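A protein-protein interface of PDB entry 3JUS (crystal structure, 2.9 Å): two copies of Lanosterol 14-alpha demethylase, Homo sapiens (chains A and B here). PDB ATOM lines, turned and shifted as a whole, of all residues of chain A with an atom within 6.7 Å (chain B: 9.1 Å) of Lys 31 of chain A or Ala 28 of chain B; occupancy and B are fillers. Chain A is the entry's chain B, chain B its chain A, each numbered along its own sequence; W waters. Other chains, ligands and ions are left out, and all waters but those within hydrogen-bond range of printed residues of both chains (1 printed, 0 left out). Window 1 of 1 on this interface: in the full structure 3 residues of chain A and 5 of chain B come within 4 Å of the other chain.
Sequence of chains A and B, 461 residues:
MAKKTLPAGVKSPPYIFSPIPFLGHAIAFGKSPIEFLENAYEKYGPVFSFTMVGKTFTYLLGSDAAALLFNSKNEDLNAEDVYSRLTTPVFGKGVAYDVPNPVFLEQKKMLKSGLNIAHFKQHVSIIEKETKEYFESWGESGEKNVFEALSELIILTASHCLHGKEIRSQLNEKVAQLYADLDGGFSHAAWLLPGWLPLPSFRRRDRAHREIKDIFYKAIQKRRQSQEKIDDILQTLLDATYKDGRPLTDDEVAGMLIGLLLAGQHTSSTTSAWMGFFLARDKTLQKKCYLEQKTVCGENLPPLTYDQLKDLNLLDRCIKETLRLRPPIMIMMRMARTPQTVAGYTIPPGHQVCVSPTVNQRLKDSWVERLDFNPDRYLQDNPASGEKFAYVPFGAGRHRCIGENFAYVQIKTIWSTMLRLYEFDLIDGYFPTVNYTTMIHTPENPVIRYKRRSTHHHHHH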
ATOM      1  N   HIS A  25     -15.206  25.457  -0.230  1.00  0.00           N
ATOM      2  CA  HIS A  25     -15.823  25.676   1.058  1.00  0.00           C
ATOM      3  C   HIS A  25     -17.336  25.464   1.008  1.00  0.00           C
ATOM      4  O   HIS A  25     -18.041  25.796   1.956  1.00  0.00           O
ATOM      5  CB  HIS A  25     -15.500  27.085   1.532  1.00  0.00           C
ATOM      6  CG  HIS A  25     -14.036  27.365   1.657  1.00  0.00           C
ATOM      7  ND1 HIS A  25     -13.334  27.146   2.825  1.00  0.00           N
ATOM      8  CD2 HIS A  25     -13.146  27.871   0.771  1.00  0.00           C
ATOM      9  CE1 HIS A  25     -12.073  27.495   2.647  1.00  0.00           C
ATOM     10  NE2 HIS A  25     -11.932  27.940   1.411  1.00  0.00           N
ATOM     11  N   ALA A  26     -17.826  24.886  -0.086  1.00  0.00           N
ATOM     12  CA  ALA A  26     -19.269  24.756  -0.307  1.00  0.00           C
ATOM     13  C   ALA A  26     -20.005  24.051   0.815  1.00  0.00           C
ATOM     14  O   ALA A  26     -21.174  24.315   1.035  1.00  0.00           O
ATOM     15  CB  ALA A  26     -19.558  24.081  -1.632  1.00  0.00           C
ATOM     16  N   ILE A  27     -19.321  23.163   1.525  1.00  0.00           N
ATOM     17  CA  ILE A  27     -19.937  22.400   2.613  1.00  0.00           C
ATOM     18  C   ILE A  27     -19.892  23.177   3.936  1.00  0.00           C
ATOM     19  O   ILE A  27     -20.903  23.289   4.623  1.00  0.00           O
ATOM     20  CB  ILE A  27     -19.293  20.996   2.749  1.00  0.00           C
ATOM     21  CG1 ILE A  27     -19.598  20.156   1.505  1.00  0.00           C
ATOM     22  CG2 ILE A  27     -19.787  20.272   3.994  1.00  0.00           C
ATOM     23  CD1 ILE A  27     -18.510  19.117   1.188  1.00  0.00           C
ATOM     24  N   ALA A  28     -18.727  23.717   4.283  1.00  0.00           N
ATOM     25  CA  ALA A  28     -18.591  24.498   5.508  1.00  0.00           C
ATOM     26  C   ALA A  28     -19.454  25.751   5.453  1.00  0.00           C
ATOM     27  O   ALA A  28     -20.162  26.063   6.411  1.00  0.00           O
ATOM     28  CB  ALA A  28     -17.143  24.861   5.756  1.00  0.00           C
ATOM     29  N   PHE A  29     -19.409  26.459   4.328  1.00  0.00           N
ATOM     30  CA  PHE A  29     -20.203  27.665   4.154  1.00  0.00           C
ATOM     31  C   PHE A  29     -21.683  27.331   4.147  1.00  0.00           C
ATOM     32  O   PHE A  29     -22.488  28.105   4.635  1.00  0.00           O
ATOM     33  CB  PHE A  29     -19.821  28.376   2.861  1.00  0.00           C
ATOM     34  CG  PHE A  29     -20.602  29.636   2.599  1.00  0.00           C
ATOM     35  CD1 PHE A  29     -20.171  30.860   3.116  1.00  0.00           C
ATOM     36  CD2 PHE A  29     -21.759  29.607   1.820  1.00  0.00           C
ATOM     37  CE1 PHE A  29     -20.885  32.030   2.868  1.00  0.00           C
ATOM     38  CE2 PHE A  29     -22.474  30.775   1.564  1.00  0.00           C
ATOM     39  CZ  PHE A  29     -22.037  31.987   2.089  1.00  0.00           C
ATOM     40  N   GLY A  30     -22.036  26.177   3.593  1.00  0.00           N
ATOM     41  CA  GLY A  30     -23.424  25.728   3.556  1.00  0.00           C
ATOM     42  C   GLY A  30     -23.988  25.435   4.935  1.00  0.00           C
ATOM     43  O   GLY A  30     -25.150  25.747   5.201  1.00  0.00           O
ATOM     44  N   LYS A  31     -23.165  24.840   5.806  1.00  0.00           N
ATOM     45  CA  LYS A  31     -23.553  24.535   7.184  1.00  0.00           C
ATOM     46  C   LYS A  31     -24.009  25.774   7.936  1.00  0.00           C
ATOM     47  O   LYS A  31     -25.186  25.902   8.255  1.00  0.00           O
ATOM     48  CB  LYS A  31     -22.421  23.837   7.954  1.00  0.00           C
ATOM     49  CG  LYS A  31     -22.531  22.302   7.982  1.00  0.00           C
ATOM     50  CD  LYS A  31     -23.965  21.816   8.331  1.00  0.00           C
ATOM     51  CE  LYS A  31     -24.198  20.358   7.910  1.00  0.00           C
ATOM     52  NZ  LYS A  31     -25.634  20.071   7.628  1.00  0.00           N
ATOM     53  N   SER A  32     -23.072  26.673   8.220  1.00  0.00           N
ATOM     54  CA  SER A  32     -23.402  27.968   8.795  1.00  0.00           C
ATOM     55  C   SER A  32     -22.607  29.087   8.144  1.00  0.00           C
ATOM     56  O   SER A  32     -21.461  29.345   8.540  1.00  0.00           O
ATOM     57  CB  SER A  32     -23.173  27.987  10.301  1.00  0.00           C
ATOM     58  OG  SER A  32     -23.462  29.283  10.812  1.00  0.00           O
ATOM     59  N   PRO A  33     -23.219  29.764   7.153  1.00  0.00           N
ATOM     60  CA  PRO A  33     -22.570  30.841   6.417  1.00  0.00           C
ATOM     61  C   PRO A  33     -22.150  31.967   7.356  1.00  0.00           C
ATOM     62  O   PRO A  33     -21.095  32.576   7.157  1.00  0.00           O
ATOM     63  CB  PRO A  33     -23.664  31.329   5.451  1.00  0.00           C
ATOM     64  CG  PRO A  33     -24.689  30.281   5.433  1.00  0.00           C
ATOM     65  CD  PRO A  33     -24.624  29.588   6.743  1.00  0.00           C
ATOM     66  N   ILE A  34     -22.965  32.218   8.379  1.00  0.00           N
ATOM     67  CA  ILE A  34     -22.696  33.278   9.345  1.00  0.00           C
ATOM     68  C   ILE A  34     -21.489  32.946  10.236  1.00  0.00           C
ATOM     69  O   ILE A  34     -20.627  33.796  10.465  1.00  0.00           O
ATOM     70  CB  ILE A  34     -23.962  33.611  10.150  1.00  0.00           C
ATOM     71  CG1 ILE A  34     -24.948  34.320   9.237  1.00  0.00           C
ATOM     72  CG2 ILE A  34     -23.655  34.532  11.308  1.00  0.00           C
ATOM     73  CD1 ILE A  34     -26.330  33.784   9.349  1.00  0.00           C
ATOM     74  N   GLU A  35     -21.431  31.703  10.705  1.00  0.00           N
ATOM     75  CA  GLU A  35     -20.286  31.176  11.435  1.00  0.00           C
ATOM     76  C   GLU A  35     -19.029  31.253  10.575  1.00  0.00           C
ATOM     77  O   GLU A  35     -17.969  31.720  11.026  1.00  0.00           O
ATOM     78  CB  GLU A  35     -20.556  29.717  11.806  1.00  0.00           C
ATOM     79  CG  GLU A  35     -19.874  29.217  13.078  1.00  0.00           C
ATOM     80  CD  GLU A  35     -20.729  28.178  13.830  1.00  0.00           C
ATOM     81  OE1 GLU A  35     -20.260  27.638  14.865  1.00  0.00           O
ATOM     82  OE2 GLU A  35     -21.878  27.913  13.392  1.00  0.00           O
ATOM     83  N   VAL A 434     -32.094  28.463  12.853  1.00  0.00           N
ATOM     84  CA  VAL A 434     -32.102  28.889  11.463  1.00  0.00           C
ATOM     85  C   VAL A 434     -31.734  27.746  10.528  1.00  0.00           C
ATOM     86  O   VAL A 434     -30.786  27.005  10.768  1.00  0.00           O
ATOM     87  CB  VAL A 434     -31.170  30.103  11.210  1.00  0.00           C
ATOM     88  CG1 VAL A 434     -31.628  30.882   9.981  1.00  0.00           C
ATOM     89  CG2 VAL A 434     -31.120  31.024  12.431  1.00  0.00           C
ATOM     90  N   TYR A 436     -30.727  26.719   6.545  1.00  0.00           N
ATOM     91  CA  TYR A 436     -30.101  27.287   5.347  1.00  0.00           C
ATOM     92  C   TYR A 436     -30.251  26.436   4.068  1.00  0.00           C
ATOM     93  O   TYR A 436     -29.697  26.786   3.018  1.00  0.00           O
ATOM     94  CB  TYR A 436     -28.641  27.638   5.627  1.00  0.00           C
ATOM     95  CG  TYR A 436     -28.486  28.671   6.719  1.00  0.00           C
ATOM     96  CD1 TYR A 436     -28.014  28.315   7.986  1.00  0.00           C
ATOM     97  CD2 TYR A 436     -28.830  30.008   6.494  1.00  0.00           C
ATOM     98  CE1 TYR A 436     -27.867  29.271   9.001  1.00  0.00           C
ATOM     99  CE2 TYR A 436     -28.698  30.972   7.503  1.00  0.00           C
ATOM    100  CZ  TYR A 436     -28.214  30.597   8.749  1.00  0.00           C
ATOM    101  OH  TYR A 436     -28.086  31.544   9.733  1.00  0.00           O
ATOM    102  N   ILE B  16     -30.414  15.701  20.672  1.00  0.00           N
ATOM    103  CA  ILE B  16     -30.311  16.682  19.608  1.00  0.00           C
ATOM    104  C   ILE B  16     -30.891  16.073  18.353  1.00  0.00           C
ATOM    105  O   ILE B  16     -30.406  15.058  17.874  1.00  0.00           O
ATOM    106  CB  ILE B  16     -28.856  17.077  19.319  1.00  0.00           C
ATOM    107  CG1 ILE B  16     -28.078  17.325  20.619  1.00  0.00           C
ATOM    108  CG2 ILE B  16     -28.823  18.281  18.384  1.00  0.00           C
ATOM    109  CD1 ILE B  16     -26.563  17.345  20.444  1.00  0.00           C
ATOM    110  N   SER B  18     -32.092  15.733  14.330  1.00  0.00           N
ATOM    111  CA  SER B  18     -31.629  16.109  13.011  1.00  0.00           C
ATOM    112  C   SER B  18     -32.743  16.007  11.977  1.00  0.00           C
ATOM    113  O   SER B  18     -33.518  15.039  11.987  1.00  0.00           O
ATOM    114  CB  SER B  18     -30.448  15.259  12.574  1.00  0.00           C
ATOM    115  OG  SER B  18     -29.928  15.784  11.365  1.00  0.00           O
ATOM    116  N   PRO B  19     -32.829  17.015  11.084  1.00  0.00           N
ATOM    117  CA  PRO B  19     -33.730  16.927   9.923  1.00  0.00           C
ATOM    118  C   PRO B  19     -33.221  15.972   8.820  1.00  0.00           C
ATOM    119  O   PRO B  19     -34.036  15.356   8.133  1.00  0.00           O
ATOM    120  CB  PRO B  19     -33.792  18.371   9.409  1.00  0.00           C
ATOM    121  CG  PRO B  19     -32.495  18.987   9.865  1.00  0.00           C
ATOM    122  CD  PRO B  19     -32.162  18.332  11.178  1.00  0.00           C
ATOM    123  N   ILE B  20     -31.901  15.841   8.661  1.00  0.00           N
ATOM    124  CA  ILE B  20     -31.326  15.012   7.589  1.00  0.00           C
ATOM    125  C   ILE B  20     -31.435  13.510   7.953  1.00  0.00           C
ATOM    126  O   ILE B  20     -30.832  13.071   8.928  1.00  0.00           O
ATOM    127  CB  ILE B  20     -29.862  15.446   7.257  1.00  0.00           C
ATOM    128  CG1 ILE B  20     -29.636  16.922   7.641  1.00  0.00           C
ATOM    129  CG2 ILE B  20     -29.541  15.183   5.773  1.00  0.00           C
ATOM    130  CD1 ILE B  20     -28.174  17.400   7.584  1.00  0.00           C
ATOM    131  N   LEU B  23     -28.145  10.296   7.530  1.00  0.00           N
ATOM    132  CA  LEU B  23     -26.885  10.933   7.881  1.00  0.00           C
ATOM    133  C   LEU B  23     -26.836  11.515   9.282  1.00  0.00           C
ATOM    134  O   LEU B  23     -25.811  11.406   9.965  1.00  0.00           O
ATOM    135  CB  LEU B  23     -26.604  12.066   6.906  1.00  0.00           C
ATOM    136  CG  LEU B  23     -25.951  11.737   5.575  1.00  0.00           C
ATOM    137  CD1 LEU B  23     -25.644  13.046   4.871  1.00  0.00           C
ATOM    138  CD2 LEU B  23     -24.682  10.912   5.782  1.00  0.00           C
ATOM    139  N   GLY B  24     -27.929  12.157   9.693  1.00  0.00           N
ATOM    140  CA  GLY B  24     -27.983  12.848  10.986  1.00  0.00           C
ATOM    141  C   GLY B  24     -27.032  14.028  11.009  1.00  0.00           C
ATOM    142  O   GLY B  24     -27.046  14.864  10.104  1.00  0.00           O
ATOM    143  N   HIS B  25     -26.182  14.083  12.026  1.00  0.00           N
ATOM    144  CA  HIS B  25     -25.236  15.186  12.173  1.00  0.00           C
ATOM    145  C   HIS B  25     -23.870  14.898  11.549  1.00  0.00           C
ATOM    146  O   HIS B  25     -22.888  15.566  11.855  1.00  0.00           O
ATOM    147  CB  HIS B  25     -25.084  15.525  13.652  1.00  0.00           C
ATOM    148  CG  HIS B  25     -26.377  15.864  14.320  1.00  0.00           C
ATOM    149  ND1 HIS B  25     -27.006  17.079  14.150  1.00  0.00           N
ATOM    150  CD2 HIS B  25     -27.166  15.144  15.149  1.00  0.00           C
ATOM    151  CE1 HIS B  25     -28.127  17.093  14.850  1.00  0.00           C
ATOM    152  NE2 HIS B  25     -28.247  15.932  15.465  1.00  0.00           N
ATOM    153  N   ALA B  26     -23.825  13.911  10.658  1.00  0.00           N
ATOM    154  CA  ALA B  26     -22.577  13.395  10.100  1.00  0.00           C
ATOM    155  C   ALA B  26     -21.671  14.477   9.549  1.00  0.00           C
ATOM    156  O   ALA B  26     -20.448  14.370   9.651  1.00  0.00           O
ATOM    157  CB  ALA B  26     -22.863  12.367   9.025  1.00  0.00           C
ATOM    158  N   ILE B  27     -22.267  15.516   8.968  1.00  0.00           N
ATOM    159  CA  ILE B  27     -21.490  16.567   8.311  1.00  0.00           C
ATOM    160  C   ILE B  27     -21.034  17.639   9.297  1.00  0.00           C
ATOM    161  O   ILE B  27     -19.864  18.021   9.297  1.00  0.00           O
ATOM    162  CB  ILE B  27     -22.250  17.173   7.102  1.00  0.00           C
ATOM    163  CG1 ILE B  27     -22.195  16.199   5.921  1.00  0.00           C
ATOM    164  CG2 ILE B  27     -21.660  18.528   6.699  1.00  0.00           C
ATOM    165  CD1 ILE B  27     -23.396  16.272   5.024  1.00  0.00           C
ATOM    166  N   ALA B  28     -21.958  18.111  10.133  1.00  0.00           N
ATOM    167  CA  ALA B  28     -21.646  19.081  11.181  1.00  0.00           C
ATOM    168  C   ALA B  28     -20.580  18.533  12.136  1.00  0.00           C
ATOM    169  O   ALA B  28     -19.601  19.220  12.452  1.00  0.00           O
ATOM    170  CB  ALA B  28     -22.915  19.480  11.940  1.00  0.00           C
ATOM    171  N   PHE B  29     -20.758  17.289  12.577  1.00  0.00           N
ATOM    172  CA  PHE B  29     -19.777  16.631  13.434  1.00  0.00           C
ATOM    173  C   PHE B  29     -18.516  16.361  12.635  1.00  0.00           C
ATOM    174  O   PHE B  29     -17.412  16.671  13.080  1.00  0.00           O
ATOM    175  CB  PHE B  29     -20.342  15.316  13.985  1.00  0.00           C
ATOM    176  CG  PHE B  29     -19.397  14.571  14.896  1.00  0.00           C
ATOM    177  CD1 PHE B  29     -19.408  14.804  16.275  1.00  0.00           C
ATOM    178  CD2 PHE B  29     -18.510  13.626  14.381  1.00  0.00           C
ATOM    179  CE1 PHE B  29     -18.543  14.113  17.126  1.00  0.00           C
ATOM    180  CE2 PHE B  29     -17.641  12.927  15.222  1.00  0.00           C
ATOM    181  CZ  PHE B  29     -17.656  13.169  16.597  1.00  0.00           C
ATOM    182  N   GLY B  30     -18.706  15.789  11.448  1.00  0.00           N
ATOM    183  CA  GLY B  30     -17.611  15.421  10.561  1.00  0.00           C
ATOM    184  C   GLY B  30     -16.626  16.546  10.337  1.00  0.00           C
ATOM    185  O   GLY B  30     -15.424  16.354  10.491  1.00  0.00           O
ATOM    186  N   LYS B  31     -17.139  17.725  10.000  1.00  0.00           N
ATOM    187  CA  LYS B  31     -16.287  18.868   9.688  1.00  0.00           C
ATOM    188  C   LYS B  31     -15.594  19.518  10.900  1.00  0.00           C
ATOM    189  O   LYS B  31     -14.496  20.061  10.760  1.00  0.00           O
ATOM    190  CB  LYS B  31     -17.043  19.913   8.854  1.00  0.00           C
ATOM    191  CG  LYS B  31     -17.159  19.562   7.353  1.00  0.00           C
ATOM    192  CD  LYS B  31     -15.842  18.998   6.760  1.00  0.00           C
ATOM    193  CE  LYS B  31     -15.537  19.589   5.380  1.00  0.00           C
ATOM    194  NZ  LYS B  31     -15.144  21.034   5.459  1.00  0.00           N
ATOM    195  N   SER B  32     -16.212  19.455  12.080  1.00  0.00           N
ATOM    196  CA  SER B  32     -15.639  20.110  13.255  1.00  0.00           C
ATOM    197  C   SER B  32     -16.200  19.564  14.574  1.00  0.00           C
ATOM    198  O   SER B  32     -17.042  20.208  15.216  1.00  0.00           O
ATOM    199  CB  SER B  32     -15.832  21.624  13.153  1.00  0.00           C
ATOM    200  OG  SER B  32     -14.807  22.282  13.870  1.00  0.00           O
ATOM    201  N   PRO B  33     -15.711  18.383  14.994  1.00  0.00           N
ATOM    202  CA  PRO B  33     -16.284  17.616  16.093  1.00  0.00           C
ATOM    203  C   PRO B  33     -16.138  18.328  17.419  1.00  0.00           C
ATOM    204  O   PRO B  33     -17.025  18.247  18.269  1.00  0.00           O
ATOM    205  CB  PRO B  33     -15.446  16.334  16.107  1.00  0.00           C
ATOM    206  CG  PRO B  33     -14.707  16.324  14.846  1.00  0.00           C
ATOM    207  CD  PRO B  33     -14.496  17.742  14.475  1.00  0.00           C
ATOM    208  N   ILE B  34     -15.017  19.016  17.585  1.00  0.00           N
ATOM    209  CA  ILE B  34     -14.730  19.744  18.805  1.00  0.00           C
ATOM    210  C   ILE B  34     -15.696  20.920  18.938  1.00  0.00           C
ATOM    211  O   ILE B  34     -16.248  21.171  20.008  1.00  0.00           O
ATOM    212  CB  ILE B  34     -13.250  20.186  18.819  1.00  0.00           C
ATOM    213  CG1 ILE B  34     -12.391  19.138  19.524  1.00  0.00           C
ATOM    214  CG2 ILE B  34     -13.075  21.543  19.497  1.00  0.00           C
ATOM    215  CD1 ILE B  34     -12.340  17.789  18.843  1.00  0.00           C
ATOM    216  N   GLU B  35     -15.909  21.608  17.822  1.00  0.00           N
ATOM    217  CA  GLU B  35     -16.831  22.725  17.743  1.00  0.00           C
ATOM    218  C   GLU B  35     -18.248  22.219  18.000  1.00  0.00           C
ATOM    219  O   GLU B  35     -18.976  22.759  18.839  1.00  0.00           O
ATOM    220  CB  GLU B  35     -16.707  23.361  16.354  1.00  0.00           C
ATOM    221  CG  GLU B  35     -17.459  24.675  16.126  1.00  0.00           C
ATOM    222  CD  GLU B  35     -17.508  25.057  14.636  1.00  0.00           C
ATOM    223  OE1 GLU B  35     -18.495  25.694  14.199  1.00  0.00           O
ATOM    224  OE2 GLU B  35     -16.559  24.715  13.890  1.00  0.00           O
ATOM    225  N   PHE B  36     -18.618  21.159  17.283  1.00  0.00           N
ATOM    226  CA  PHE B  36     -19.929  20.550  17.424  1.00  0.00           C
ATOM    227  C   PHE B  36     -20.205  20.201  18.879  1.00  0.00           C
ATOM    228  O   PHE B  36     -21.273  20.518  19.391  1.00  0.00           O
ATOM    229  CB  PHE B  36     -20.032  19.305  16.540  1.00  0.00           C
ATOM    230  CG  PHE B  36     -21.390  18.642  16.567  1.00  0.00           C
ATOM    231  CD1 PHE B  36     -22.255  18.764  15.482  1.00  0.00           C
ATOM    232  CD2 PHE B  36     -21.799  17.876  17.664  1.00  0.00           C
ATOM    233  CE1 PHE B  36     -23.512  18.151  15.493  1.00  0.00           C
ATOM    234  CE2 PHE B  36     -23.045  17.266  17.680  1.00  0.00           C
ATOM    235  CZ  PHE B  36     -23.906  17.409  16.588  1.00  0.00           C
ATOM    236  N   LEU B  37     -19.233  19.567  19.537  1.00  0.00           N
ATOM    237  CA  LEU B  37     -19.396  19.067  20.904  1.00  0.00           C
ATOM    238  C   LEU B  37     -19.380  20.171  21.945  1.00  0.00           C
ATOM    239  O   LEU B  37     -20.142  20.133  22.899  1.00  0.00           O
ATOM    240  CB  LEU B  37     -18.331  18.012  21.242  1.00  0.00           C
ATOM    241  CG  LEU B  37     -18.387  16.638  20.564  1.00  0.00           C
ATOM    242  CD1 LEU B  37     -17.259  15.774  21.064  1.00  0.00           C
ATOM    243  CD2 LEU B  37     -19.722  15.982  20.825  1.00  0.00           C
ATOM    244  N   ASN B  39     -20.228  23.350  21.307  1.00  0.00           N
ATOM    245  CA  ASN B  39     -21.536  23.983  21.058  1.00  0.00           C
ATOM    246  C   ASN B  39     -22.681  23.246  21.739  1.00  0.00           C
ATOM    247  O   ASN B  39     -23.488  23.852  22.458  1.00  0.00           O
ATOM    248  CB  ASN B  39     -21.824  24.114  19.557  1.00  0.00           C
ATOM    249  CG  ASN B  39     -21.092  25.294  18.923  1.00  0.00           C
ATOM    250  OD1 ASN B  39     -20.746  26.266  19.607  1.00  0.00           O
ATOM    251  ND2 ASN B  39     -20.842  25.210  17.614  1.00  0.00           N
ATOM    252  N   PHE B  50     -26.955  12.123  20.180  1.00  0.00           N
ATOM    253  CA  PHE B  50     -27.295  12.406  18.787  1.00  0.00           C
ATOM    254  C   PHE B  50     -27.047  11.206  17.905  1.00  0.00           C
ATOM    255  O   PHE B  50     -26.342  10.285  18.293  1.00  0.00           O
ATOM    256  CB  PHE B  50     -26.550  13.637  18.253  1.00  0.00           C
ATOM    257  CG  PHE B  50     -25.053  13.563  18.386  1.00  0.00           C
ATOM    258  CD1 PHE B  50     -24.261  13.301  17.276  1.00  0.00           C
ATOM    259  CD2 PHE B  50     -24.434  13.785  19.618  1.00  0.00           C
ATOM    260  CE1 PHE B  50     -22.864  13.246  17.388  1.00  0.00           C
ATOM    261  CE2 PHE B  50     -23.050  13.736  19.743  1.00  0.00           C
ATOM    262  CZ  PHE B  50     -22.260  13.465  18.624  1.00  0.00           C
ATOM    263  N   THR B  51     -27.642  11.217  16.720  1.00  0.00           N
ATOM    264  CA  THR B  51     -27.496  10.106  15.785  1.00  0.00           C
ATOM    265  C   THR B  51     -26.689  10.511  14.556  1.00  0.00           C
ATOM    266  O   THR B  51     -26.747  11.654  14.105  1.00  0.00           O
ATOM    267  CB  THR B  51     -28.865   9.498  15.354  1.00  0.00           C
ATOM    268  OG1 THR B  51     -29.755  10.542  14.960  1.00  0.00           O
ATOM    269  CG2 THR B  51     -29.514   8.749  16.486  1.00  0.00           C
ATOM    270  N   MET B  52     -25.929   9.547  14.038  1.00  0.00           N
ATOM    271  CA  MET B  52     -25.057   9.718  12.877  1.00  0.00           C
ATOM    272  C   MET B  52     -24.987   8.409  12.106  1.00  0.00           C
ATOM    273  O   MET B  52     -24.613   7.366  12.668  1.00  0.00           O
ATOM    274  CB  MET B  52     -23.644  10.113  13.315  1.00  0.00           C
ATOM    275  CG  MET B  52     -23.355  11.596  13.351  1.00  0.00           C
ATOM    276  SD  MET B  52     -21.827  11.945  14.254  1.00  0.00           S
ATOM    277  CE  MET B  52     -20.587  11.078  13.291  1.00  0.00           C
ATOM    278  N   TYR B 436      -9.412  16.775  10.296  1.00  0.00           N
ATOM    279  CA  TYR B 436     -10.200  15.793  11.036  1.00  0.00           C
ATOM    280  C   TYR B 436     -10.688  14.615  10.205  1.00  0.00           C
ATOM    281  O   TYR B 436     -11.239  13.662  10.767  1.00  0.00           O
ATOM    282  CB  TYR B 436     -11.405  16.468  11.704  1.00  0.00           C
ATOM    283  CG  TYR B 436     -11.063  17.383  12.859  1.00  0.00           C
ATOM    284  CD1 TYR B 436     -11.358  18.748  12.802  1.00  0.00           C
ATOM    285  CD2 TYR B 436     -10.446  16.883  14.014  1.00  0.00           C
ATOM    286  CE1 TYR B 436     -11.050  19.592  13.866  1.00  0.00           C
ATOM    287  CE2 TYR B 436     -10.131  17.718  15.080  1.00  0.00           C
ATOM    288  CZ  TYR B 436     -10.435  19.069  15.000  1.00  0.00           C
ATOM    289  OH  TYR B 436     -10.119  19.893  16.058  1.00  0.00           O
HETATM  290  O   HOH W   1     -25.008  16.924   8.874  1.00  0.00           O
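The side-chain carboxylate (OE1) of Glu 35 of chain A sits close to the side-chain carboxylate (OE1) of Glu 35 of chain B (2.7 Å).
The backbone NH of Ile 20 of chain B sits at hydrogen-bond distance from the side-chain hydroxyl of Ser 18 of chain B (3.3 Å).
The side-chain carboxylate of Glu 35 of chain B lies within hydrogen-bond range of the side-chain hydroxyl of Ser 32 of chain B, 3.0 Å away.
O of Glu 35 of chain B lies close to ND2 of Asn 39 of chain B (3.3 Å).
OG of Ser 32 of chain A sits close to N of Glu 35 of chain A (3.2 Å).
Ile 27 of chain A touches Ile 27 of chain B.
NZ of Lys 31 of chain A touches CD1 of Ile 20 of chain B (3.7 Å).
CE of Lys 31 of chain A touches CG2 of Ile 27 of chain B (3.4 Å).
Lys 31 of chain A touches Ala 28 of chain B.
ND2 of Asn 39 of chain B touches OE1 of Glu 35 of chain A (3.7 Å).
Lys 31 of chain A touches just these residues of chain B: Ile 20, Ile 27 and Ala 28.
Ala 28 of chain B touches one residue of chain A.
No residue of chain B comes within 4 Å of Gly 30 of chain A.
No residue of chain B comes within 4 Å of Ser 32 of chain A.
Of the printed residues of chain B, Ile 27 of chain A touches Ile 27 (3.7 Å).
Printed residues of chain A within 4 Å of Ile 20 of chain B: Lys 31.
Printed residues of chain B within 4 Å of Glu 35 of chain A: Glu 35 and Asn 39.
Printed residues of chain A within 4 Å of Asn 39 of chain B: Glu 35.
Printed residues of chain A within 4 Å of Ile 27 of chain B: Ile 27 (3.7 Å) and Lys 31 (3.4 Å).
Hydrophobic or aromatic side chains of chain B within 4 Å of the printed part of chain A: Ile 20 and Ile 27.
Of the 13 printed residues of chain A, 3 touch a printed residue of chain B.
Along chain A the printed residues that touch a printed residue of chain B span positions 27 to 35.
Among the printed residues, no Asp or Glu carboxylate lies within 4 Å of a Lys or Arg side-chain nitrogen of the other chain.
Ile 27 of chain A touches its own counterpart, Ile 27 of chain B.
Lys 31 of chain A touches Ile 27 of chain B, but with the chains exchanged Ile 27 of chain A does not touch Lys 31 of chain B (4.3 Å).
Lys 31 of chain A touches Ala 28 of chain B, but with the chains exchanged Ala 28 of chain A does not touch Lys 31 of chain B (4.3 Å).
Glu 35 of chain B touches its own counterpart, Glu 35 of chain A.
Positions printed for both chains: 25, 26, 27, 28, 29, 30, 31, 32, 33, 34, 35 and 436.
Of the 6 pairs that touch across the chains among the printed residues, 2 have their exchanged pair printed and touching as well.
Water W1 lies within hydrogen-bond range of the backbone NH (N) of Ile 27 of chain B (3.1 Å), the backbone carbonyl oxygen (O) of Gly 24 of chain B (3.1 Å) and the side-chain amino group (NZ) of Lys 31 of chain A (3.4 Å).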
